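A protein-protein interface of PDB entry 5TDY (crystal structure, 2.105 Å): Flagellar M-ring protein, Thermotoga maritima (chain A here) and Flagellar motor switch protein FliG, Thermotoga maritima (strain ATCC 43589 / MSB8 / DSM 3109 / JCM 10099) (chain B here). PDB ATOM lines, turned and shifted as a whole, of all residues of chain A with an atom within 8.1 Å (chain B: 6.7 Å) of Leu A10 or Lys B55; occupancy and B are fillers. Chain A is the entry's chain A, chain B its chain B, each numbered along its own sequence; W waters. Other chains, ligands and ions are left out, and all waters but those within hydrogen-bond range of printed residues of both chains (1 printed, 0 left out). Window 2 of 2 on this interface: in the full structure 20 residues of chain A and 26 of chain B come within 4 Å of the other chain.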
ATOM      1  N   GLU A   3       2.817  23.264   5.562  1.00  0.00           N
ATOM      2  CA  GLU A   3       3.246  23.837   6.832  1.00  0.00           C
ATOM      3  C   GLU A   3       2.966  22.872   7.981  1.00  0.00           C
ATOM      4  O   GLU A   3       3.769  22.753   8.913  1.00  0.00           O
ATOM      5  CB  GLU A   3       2.544  25.178   7.068  1.00  0.00           C
ATOM      6  CG  GLU A   3       2.556  26.125   5.867  1.00  0.00           C
ATOM      7  CD  GLU A   3       1.449  25.834   4.852  1.00  0.00           C
ATOM      8  OE1 GLU A   3       0.257  25.998   5.198  1.00  0.00           O
ATOM      9  OE2 GLU A   3       1.773  25.427   3.708  1.00  0.00           O
ATOM     10  N   GLU A   4       1.837  22.164   7.930  1.00  0.00           N
ATOM     11  CA  GLU A   4       1.589  21.149   8.947  1.00  0.00           C
ATOM     12  C   GLU A   4       2.615  20.026   8.858  1.00  0.00           C
ATOM     13  O   GLU A   4       3.080  19.533   9.889  1.00  0.00           O
ATOM     14  CB  GLU A   4       0.156  20.606   8.831  1.00  0.00           C
ATOM     15  CG  GLU A   4      -0.901  21.615   9.301  1.00  0.00           C
ATOM     16  CD  GLU A   4      -2.349  21.210   9.017  1.00  0.00           C
ATOM     17  OE1 GLU A   4      -3.251  21.852   9.605  1.00  0.00           O
ATOM     18  OE2 GLU A   4      -2.596  20.275   8.220  1.00  0.00           O
ATOM     19  N   LYS A   5       3.017  19.648   7.643  1.00  0.00           N
ATOM     20  CA  LYS A   5       3.984  18.567   7.479  1.00  0.00           C
ATOM     21  C   LYS A   5       5.305  18.893   8.165  1.00  0.00           C
ATOM     22  O   LYS A   5       5.897  18.033   8.828  1.00  0.00           O
ATOM     23  CB  LYS A   5       4.205  18.283   5.991  1.00  0.00           C
ATOM     24  CG  LYS A   5       5.402  17.399   5.684  1.00  0.00           C
ATOM     25  CD  LYS A   5       5.979  17.693   4.296  1.00  0.00           C
ATOM     26  CE  LYS A   5       7.301  16.964   4.085  1.00  0.00           C
ATOM     27  NZ  LYS A   5       7.563  16.679   2.641  1.00  0.00           N
ATOM     28  N   GLU A   6       5.785  20.131   8.027  1.00  0.00           N
ATOM     29  CA  GLU A   6       7.037  20.483   8.683  1.00  0.00           C
ATOM     30  C   GLU A   6       6.872  20.637  10.190  1.00  0.00           C
ATOM     31  O   GLU A   6       7.851  20.465  10.925  1.00  0.00           O
ATOM     32  CB  GLU A   6       7.625  21.750   8.065  1.00  0.00           C
ATOM     33  CG  GLU A   6       7.076  23.048   8.600  1.00  0.00           C
ATOM     34  CD  GLU A   6       7.808  24.249   8.025  1.00  0.00           C
ATOM     35  OE1 GLU A   6       7.236  25.356   8.065  1.00  0.00           O
ATOM     36  OE2 GLU A   6       8.951  24.089   7.532  1.00  0.00           O
ATOM     37  N   LEU A   7       5.658  20.911  10.670  1.00  0.00           N
ATOM     38  CA  LEU A   7       5.426  20.901  12.110  1.00  0.00           C
ATOM     39  C   LEU A   7       5.600  19.497  12.684  1.00  0.00           C
ATOM     40  O   LEU A   7       6.276  19.320  13.709  1.00  0.00           O
ATOM     41  CB  LEU A   7       4.039  21.457  12.434  1.00  0.00           C
ATOM     42  CG  LEU A   7       3.701  21.339  13.924  1.00  0.00           C
ATOM     43  CD1 LEU A   7       4.680  22.175  14.750  1.00  0.00           C
ATOM     44  CD2 LEU A   7       2.252  21.742  14.210  1.00  0.00           C
ATOM     45  N   LEU A   8       5.006  18.479  12.036  1.00  0.00           N
ATOM     46  CA  LEU A   8       5.201  17.107  12.511  1.00  0.00           C
ATOM     47  C   LEU A   8       6.662  16.711  12.478  1.00  0.00           C
ATOM     48  O   LEU A   8       7.100  15.900  13.300  1.00  0.00           O
ATOM     49  CB  LEU A   8       4.421  16.071  11.692  1.00  0.00           C
ATOM     50  CG  LEU A   8       2.906  15.890  11.629  1.00  0.00           C
ATOM     51  CD1 LEU A   8       2.276  15.991  13.012  1.00  0.00           C
ATOM     52  CD2 LEU A   8       2.253  16.807  10.633  1.00  0.00           C
ATOM     53  N   GLU A   9       7.415  17.233  11.507  1.00  0.00           N
ATOM     54  CA  GLU A   9       8.840  16.951  11.452  1.00  0.00           C
ATOM     55  C   GLU A   9       9.540  17.505  12.682  1.00  0.00           C
ATOM     56  O   GLU A   9      10.345  16.813  13.319  1.00  0.00           O
ATOM     57  CB  GLU A   9       9.444  17.537  10.173  1.00  0.00           C
ATOM     58  CG  GLU A   9       9.038  16.811   8.898  1.00  0.00           C
ATOM     59  CD  GLU A   9       9.918  17.196   7.721  1.00  0.00           C
ATOM     60  OE1 GLU A   9      10.234  18.400   7.580  1.00  0.00           O
ATOM     61  OE2 GLU A   9      10.310  16.294   6.947  1.00  0.00           O
ATOM     62  N   LEU A  10       9.245  18.761  13.028  1.00  0.00           N
ATOM     63  CA  LEU A  10       9.818  19.348  14.235  1.00  0.00           C
ATOM     64  C   LEU A  10       9.372  18.590  15.477  1.00  0.00           C
ATOM     65  O   LEU A  10      10.177  18.331  16.378  1.00  0.00           O
ATOM     66  CB  LEU A  10       9.424  20.819  14.340  1.00  0.00           C
ATOM     67  CG  LEU A  10       9.977  21.764  13.276  1.00  0.00           C
ATOM     68  CD1 LEU A  10       9.205  23.071  13.302  1.00  0.00           C
ATOM     69  CD2 LEU A  10      11.454  22.011  13.525  1.00  0.00           C
ATOM     70  N   LEU A  11       8.089  18.220  15.545  1.00  0.00           N
ATOM     71  CA  LEU A  11       7.609  17.460  16.695  1.00  0.00           C
ATOM     72  C   LEU A  11       8.290  16.100  16.793  1.00  0.00           C
ATOM     73  O   LEU A  11       8.565  15.622  17.902  1.00  0.00           O
ATOM     74  CB  LEU A  11       6.089  17.305  16.622  1.00  0.00           C
ATOM     75  CG  LEU A  11       5.368  18.639  16.838  1.00  0.00           C
ATOM     76  CD1 LEU A  11       3.916  18.570  16.442  1.00  0.00           C
ATOM     77  CD2 LEU A  11       5.530  19.116  18.285  1.00  0.00           C
ATOM     78  N   GLU A  12       8.593  15.466  15.656  1.00  0.00           N
ATOM     79  CA  GLU A  12       9.270  14.172  15.715  1.00  0.00           C
ATOM     80  C   GLU A  12      10.665  14.311  16.308  1.00  0.00           C
ATOM     81  O   GLU A  12      11.057  13.527  17.184  1.00  0.00           O
ATOM     82  CB  GLU A  12       9.338  13.516  14.329  1.00  0.00           C
ATOM     83  CG  GLU A  12      10.320  12.343  14.295  1.00  0.00           C
ATOM     84  CD  GLU A  12      10.234  11.502  13.044  1.00  0.00           C
ATOM     85  OE1 GLU A  12      10.704  10.344  13.102  1.00  0.00           O
ATOM     86  OE2 GLU A  12       9.715  11.997  12.019  1.00  0.00           O
ATOM     87  N   GLU A  13      11.422  15.330  15.872  1.00  0.00           N
ATOM     88  CA  GLU A  13      12.716  15.609  16.490  1.00  0.00           C
ATOM     89  C   GLU A  13      12.578  15.877  17.983  1.00  0.00           C
ATOM     90  O   GLU A  13      13.403  15.424  18.778  1.00  0.00           O
ATOM     91  CB  GLU A  13      13.389  16.806  15.817  1.00  0.00           C
ATOM     92  CG  GLU A  13      13.712  16.619  14.348  1.00  0.00           C
ATOM     93  CD  GLU A  13      15.174  16.884  14.037  1.00  0.00           C
ATOM     94  OE1 GLU A  13      15.908  17.363  14.937  1.00  0.00           O
ATOM     95  OE2 GLU A  13      15.590  16.620  12.888  1.00  0.00           O
ATOM     96  N   LEU A  14      11.573  16.663  18.380  1.00  0.00           N
ATOM     97  CA  LEU A  14      11.348  16.906  19.801  1.00  0.00           C
ATOM     98  C   LEU A  14      11.105  15.596  20.539  1.00  0.00           C
ATOM     99  O   LEU A  14      11.701  15.340  21.593  1.00  0.00           O
ATOM    100  CB  LEU A  14      10.162  17.854  19.999  1.00  0.00           C
ATOM    101  CG  LEU A  14       9.692  18.062  21.448  1.00  0.00           C
ATOM    102  CD1 LEU A  14      10.811  18.686  22.267  1.00  0.00           C
ATOM    103  CD2 LEU A  14       8.446  18.942  21.484  1.00  0.00           C
ATOM    104  N   GLU A  15      10.235  14.751  19.982  1.00  0.00           N
ATOM    105  CA  GLU A  15       9.962  13.444  20.573  1.00  0.00           C
ATOM    106  C   GLU A  15      11.243  12.634  20.729  1.00  0.00           C
ATOM    107  O   GLU A  15      11.500  12.058  21.793  1.00  0.00           O
ATOM    108  CB  GLU A  15       8.947  12.693  19.707  1.00  0.00           C
ATOM    109  CG  GLU A  15       7.500  13.137  19.879  1.00  0.00           C
ATOM    110  CD  GLU A  15       6.526  12.255  19.098  1.00  0.00           C
ATOM    111  OE1 GLU A  15       6.984  11.464  18.238  1.00  0.00           O
ATOM    112  OE2 GLU A  15       5.305  12.358  19.352  1.00  0.00           O
ATOM    113  N   ASN A  16      12.067  12.613  19.698  1.00  0.00           N
ATOM    114  CA  ASN A  16      13.299  11.889  19.722  1.00  0.00           C
ATOM    115  C   ASN A  16      14.227  12.386  20.856  1.00  0.00           C
ATOM    116  O   ASN A  16      14.811  11.629  21.521  1.00  0.00           O
ATOM    117  CB  ASN A  16      13.937  11.921  18.348  1.00  0.00           C
ATOM    118  CG  ASN A  16      13.308  10.914  17.383  1.00  0.00           C
ATOM    119  OD1 ASN A  16      12.127  10.821  17.221  1.00  0.00           O
ATOM    120  ND2 ASN A  16      14.126  10.155  16.771  1.00  0.00           N
ATOM    121  N   ILE A  17      14.309  13.680  21.042  1.00  0.00           N
ATOM    122  CA  ILE A  17      15.085  14.247  22.096  1.00  0.00           C
ATOM    123  C   ILE A  17      14.565  13.823  23.468  1.00  0.00           C
ATOM    124  O   ILE A  17      15.332  13.534  24.322  1.00  0.00           O
ATOM    125  CB  ILE A  17      15.229  15.764  21.943  1.00  0.00           C
ATOM    126  CG1 ILE A  17      16.148  16.046  20.773  1.00  0.00           C
ATOM    127  CG2 ILE A  17      15.839  16.376  23.177  1.00  0.00           C
ATOM    128  CD1 ILE A  17      16.285  17.487  20.414  1.00  0.00           C
ATOM    129  N   VAL B  14       5.372  27.453  25.806  1.00  0.00           N
ATOM    130  CA  VAL B  14       4.982  26.898  24.515  1.00  0.00           C
ATOM    131  C   VAL B  14       5.599  25.517  24.325  1.00  0.00           C
ATOM    132  O   VAL B  14       4.938  24.585  23.840  1.00  0.00           O
ATOM    133  CB  VAL B  14       5.360  27.868  23.375  1.00  0.00           C
ATOM    134  CG1 VAL B  14       5.218  27.187  21.997  1.00  0.00           C
ATOM    135  CG2 VAL B  14       4.492  29.145  23.439  1.00  0.00           C
ATOM    136  N   VAL B  49      -1.841  29.674  21.234  1.00  0.00           N
ATOM    137  CA  VAL B  49      -0.499  29.581  20.668  1.00  0.00           C
ATOM    138  C   VAL B  49      -0.643  29.617  19.151  1.00  0.00           C
ATOM    139  O   VAL B  49      -1.340  28.780  18.573  1.00  0.00           O
ATOM    140  CB  VAL B  49       0.232  28.306  21.127  1.00  0.00           C
ATOM    141  CG1 VAL B  49       1.571  28.153  20.393  1.00  0.00           C
ATOM    142  CG2 VAL B  49       0.475  28.324  22.625  1.00  0.00           C
ATOM    143  N   THR B  50      -0.007  30.593  18.503  1.00  0.00           N
ATOM    144  CA  THR B  50      -0.117  30.650  17.055  1.00  0.00           C
ATOM    145  C   THR B  50       0.766  29.579  16.425  1.00  0.00           C
ATOM    146  O   THR B  50       1.721  29.106  17.048  1.00  0.00           O
ATOM    147  CB  THR B  50       0.266  32.035  16.545  1.00  0.00           C
ATOM    148  OG1 THR B  50       1.638  32.312  16.847  1.00  0.00           O
ATOM    149  CG2 THR B  50      -0.622  33.102  17.185  1.00  0.00           C
ATOM    150  N   PRO B  51       0.450  29.148  15.199  1.00  0.00           N
ATOM    151  CA  PRO B  51       1.327  28.171  14.533  1.00  0.00           C
ATOM    152  C   PRO B  51       2.747  28.677  14.354  1.00  0.00           C
ATOM    153  O   PRO B  51       3.694  27.879  14.401  1.00  0.00           O
ATOM    154  CB  PRO B  51       0.637  27.933  13.179  1.00  0.00           C
ATOM    155  CG  PRO B  51      -0.770  28.400  13.363  1.00  0.00           C
ATOM    156  CD  PRO B  51      -0.699  29.522  14.356  1.00  0.00           C
ATOM    157  N   GLU B  52       2.919  29.990  14.175  1.00  0.00           N
ATOM    158  CA  GLU B  52       4.245  30.556  13.969  1.00  0.00           C
ATOM    159  C   GLU B  52       5.041  30.614  15.266  1.00  0.00           C
ATOM    160  O   GLU B  52       6.250  30.368  15.257  1.00  0.00           O
ATOM    161  CB  GLU B  52       4.143  31.956  13.362  1.00  0.00           C
ATOM    162  CG  GLU B  52       3.560  32.002  11.965  1.00  0.00           C
ATOM    163  CD  GLU B  52       2.049  31.935  11.947  1.00  0.00           C
ATOM    164  OE1 GLU B  52       1.488  31.639  10.871  1.00  0.00           O
ATOM    165  OE2 GLU B  52       1.419  32.166  13.006  1.00  0.00           O
ATOM    166  N   GLU B  53       4.391  30.989  16.374  1.00  0.00           N
ATOM    167  CA  GLU B  53       5.017  30.876  17.686  1.00  0.00           C
ATOM    168  C   GLU B  53       5.528  29.461  17.906  1.00  0.00           C
ATOM    169  O   GLU B  53       6.702  29.249  18.233  1.00  0.00           O
ATOM    170  CB  GLU B  53       4.018  31.253  18.779  1.00  0.00           C
ATOM    171  CG  GLU B  53       4.268  32.586  19.439  1.00  0.00           C
ATOM    172  CD  GLU B  53       3.137  32.990  20.382  1.00  0.00           C
ATOM    173  OE1 GLU B  53       3.293  34.018  21.079  1.00  0.00           O
ATOM    174  OE2 GLU B  53       2.088  32.297  20.412  1.00  0.00           O
ATOM    175  N   LYS B  54       4.653  28.477  17.698  1.00  0.00           N
ATOM    176  CA  LYS B  54       5.003  27.084  17.959  1.00  0.00           C
ATOM    177  C   LYS B  54       6.208  26.654  17.135  1.00  0.00           C
ATOM    178  O   LYS B  54       7.147  26.043  17.659  1.00  0.00           O
ATOM    179  CB  LYS B  54       3.802  26.199  17.652  1.00  0.00           C
ATOM    180  CG  LYS B  54       3.895  24.788  18.162  1.00  0.00           C
ATOM    181  CD  LYS B  54       2.482  24.206  18.258  1.00  0.00           C
ATOM    182  CE  LYS B  54       2.483  22.845  18.920  1.00  0.00           C
ATOM    183  NZ  LYS B  54       1.125  22.227  18.985  1.00  0.00           N
ATOM    184  N   LYS B  55       6.189  26.961  15.838  1.00  0.00           N
ATOM    185  CA  LYS B  55       7.291  26.606  14.947  1.00  0.00           C
ATOM    186  C   LYS B  55       8.581  27.330  15.333  1.00  0.00           C
ATOM    187  O   LYS B  55       9.662  26.730  15.316  1.00  0.00           O
ATOM    188  CB  LYS B  55       6.890  26.934  13.507  1.00  0.00           C
ATOM    189  CG  LYS B  55       7.815  26.420  12.423  1.00  0.00           C
ATOM    190  CD  LYS B  55       7.314  26.906  11.054  1.00  0.00           C
ATOM    191  CE  LYS B  55       8.471  27.170  10.051  1.00  0.00           C
ATOM    192  NZ  LYS B  55       9.445  28.212  10.477  1.00  0.00           N
ATOM    193  N   GLN B  56       8.486  28.618  15.686  1.00  0.00           N
ATOM    194  CA  GLN B  56       9.666  29.361  16.127  1.00  0.00           C
ATOM    195  C   GLN B  56      10.269  28.749  17.383  1.00  0.00           C
ATOM    196  O   GLN B  56      11.491  28.565  17.476  1.00  0.00           O
ATOM    197  CB  GLN B  56       9.316  30.822  16.397  1.00  0.00           C
ATOM    198  CG  GLN B  56       9.166  31.710  15.180  1.00  0.00           C
ATOM    199  CD  GLN B  56       8.716  33.113  15.561  1.00  0.00           C
ATOM    200  OE1 GLN B  56       7.666  33.583  15.117  1.00  0.00           O
ATOM    201  NE2 GLN B  56       9.507  33.787  16.390  1.00  0.00           N
ATOM    202  N   VAL B  57       9.434  28.462  18.381  1.00  0.00           N
ATOM    203  CA  VAL B  57       9.952  27.893  19.621  1.00  0.00           C
ATOM    204  C   VAL B  57      10.613  26.550  19.347  1.00  0.00           C
ATOM    205  O   VAL B  57      11.722  26.271  19.828  1.00  0.00           O
ATOM    206  CB  VAL B  57       8.828  27.778  20.668  1.00  0.00           C
ATOM    207  CG1 VAL B  57       9.298  26.968  21.875  1.00  0.00           C
ATOM    208  CG2 VAL B  57       8.361  29.160  21.093  1.00  0.00           C
ATOM    209  N   LEU B  58       9.972  25.718  18.531  1.00  0.00           N
ATOM    210  CA  LEU B  58      10.522  24.395  18.264  1.00  0.00           C
ATOM    211  C   LEU B  58      11.858  24.487  17.530  1.00  0.00           C
ATOM    212  O   LEU B  58      12.794  23.737  17.833  1.00  0.00           O
ATOM    213  CB  LEU B  58       9.513  23.567  17.471  1.00  0.00           C
ATOM    214  CG  LEU B  58       8.304  23.123  18.303  1.00  0.00           C
ATOM    215  CD1 LEU B  58       7.321  22.323  17.452  1.00  0.00           C
ATOM    216  CD2 LEU B  58       8.736  22.314  19.520  1.00  0.00           C
ATOM    217  N   GLU B  59      11.977  25.423  16.580  1.00  0.00           N
ATOM    218  CA  GLU B  59      13.233  25.577  15.836  1.00  0.00           C
ATOM    219  C   GLU B  59      14.383  26.004  16.738  1.00  0.00           C
ATOM    220  O   GLU B  59      15.488  25.451  16.649  1.00  0.00           O
ATOM    221  CB  GLU B  59      13.054  26.583  14.700  1.00  0.00           C
ATOM    222  CG  GLU B  59      12.410  25.941  13.495  1.00  0.00           C
ATOM    223  CD  GLU B  59      11.692  26.925  12.631  1.00  0.00           C
ATOM    224  OE1 GLU B  59      11.000  26.479  11.693  1.00  0.00           O
ATOM    225  OE2 GLU B  59      11.822  28.141  12.885  1.00  0.00           O
ATOM    226  N   GLU B  60      14.147  26.998  17.598  1.00  0.00           N
ATOM    227  CA  GLU B  60      15.179  27.426  18.533  1.00  0.00           C
ATOM    228  C   GLU B  60      15.518  26.315  19.521  1.00  0.00           C
ATOM    229  O   GLU B  60      16.696  26.074  19.813  1.00  0.00           O
ATOM    230  CB  GLU B  60      14.734  28.697  19.275  1.00  0.00           C
ATOM    231  CG  GLU B  60      15.855  29.268  20.156  1.00  0.00           C
ATOM    232  CD  GLU B  60      15.456  30.489  20.990  1.00  0.00           C
ATOM    233  OE1 GLU B  60      14.435  31.146  20.710  1.00  0.00           O
ATOM    234  OE2 GLU B  60      16.194  30.806  21.943  1.00  0.00           O
ATOM    235  N   LEU B  62      15.452  23.073  19.108  1.00  0.00           N
ATOM    236  CA  LEU B  62      16.253  22.018  18.491  1.00  0.00           C
ATOM    237  C   LEU B  62      17.705  22.449  18.306  1.00  0.00           C
ATOM    238  O   LEU B  62      18.632  21.674  18.592  1.00  0.00           O
ATOM    239  CB  LEU B  62      15.636  21.608  17.150  1.00  0.00           C
ATOM    240  CG  LEU B  62      14.356  20.763  17.274  1.00  0.00           C
ATOM    241  CD1 LEU B  62      13.710  20.531  15.920  1.00  0.00           C
ATOM    242  CD2 LEU B  62      14.622  19.425  17.962  1.00  0.00           C
ATOM    243  N   LYS B  85      14.680  25.624   2.220  1.00  0.00           N
ATOM    244  CA  LYS B  85      13.954  26.600   3.032  1.00  0.00           C
ATOM    245  C   LYS B  85      14.240  28.028   2.583  1.00  0.00           C
ATOM    246  O   LYS B  85      13.352  28.894   2.627  1.00  0.00           O
ATOM    247  CB  LYS B  85      14.309  26.432   4.506  1.00  0.00           C
ATOM    248  CG  LYS B  85      13.756  25.161   5.132  1.00  0.00           C
ATOM    249  CD  LYS B  85      14.313  24.995   6.547  1.00  0.00           C
ATOM    250  CE  LYS B  85      13.962  23.629   7.135  1.00  0.00           C
ATOM    251  NZ  LYS B  85      12.497  23.481   7.298  1.00  0.00           N
HETATM  252  O   HOH W   1      11.242  25.432   8.319  1.00  0.00           O
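Among the printed residues, pairs that only touch across the chains: Glu A6 with Lys B55 (3.0 Å), Leu A7 with Leu B58 (3.8 Å), Leu A10 with Lys B55 (3.7 Å), Leu A10 with Leu B62 (3.6 Å), Leu A11 with Leu B58 (3.8 Å), Glu A13 with Leu B62 (3.6 Å), Leu A14 with Leu B58 (3.9 Å) and Ile A17 with Leu B62 (3.5 Å).
Of the printed residues of chain B, Glu A6 touches Lys B55 (3.0 Å) and Lys B85 (3.6 Å). Of the printed residues of chain B, Ile A17 touches Leu B62. Glu B52 touches none of the printed residues of chain A. Lys B54 touches none of the printed residues of chain A. Lys B55 touches just these residues of chain A: Glu A6 (3.0 Å) and Leu A10 (3.7 Å). Of the printed residues of chain A, Leu B58 touches Leu A7 (3.8 Å), Leu A11 (3.8 Å) and Leu A14 (3.9 Å). Of the printed residues of chain A, Leu B62 touches Leu A10 (3.6 Å), Glu A13 (3.6 Å) and Ile A17 (3.5 Å). Of the printed residues of chain A, Lys B85 touches Glu A6 (3.6 Å). The nearest printed residue of chain B that does not touch Leu A10 is Glu B59 (4.04 Å). The nearest printed residue of chain B that does not touch Leu A7 is Lys B54 (4.4 Å).
The side-chain amino group (NZ) of Lys B85 lies within salt-bridge range of the side-chain carboxylate (OE2) of Glu A6 (3.6 Å).
Of the 15 printed residues of chain B, 4 touch a printed residue of chain A. Printed residues of chain B that touch a printed residue of chain A: Lys B55, Leu B58, Leu B62 and Lys B85. Hydrophobic or aromatic side chains of chain B within 4 Å of the printed part of chain A: Leu B58 and Leu B62. Of the 15 printed residues of chain A, 7 touch a printed residue of chain B. Hydrophobic or aromatic side chains of chain A that line the printed part of chain B: Leu A7, Leu A10, Leu A11, Leu A14 and Ile A17. Among the printed residues, Asp or Glu carboxylates within 4 Å of a Lys or Arg side-chain nitrogen of the other chain: Glu A6 with Lys B85 (3.6 Å).
The side-chain amino group of Lys B55 lies within salt-bridge range of the side-chain carboxylate of Glu B59, 2.6 Å away.
Water W1 bridges the side-chain amino group (NZ) of Lys B85 (2.5 Å) and the side-chain carboxylate (OE2) of Glu A6 (2.8 Å).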
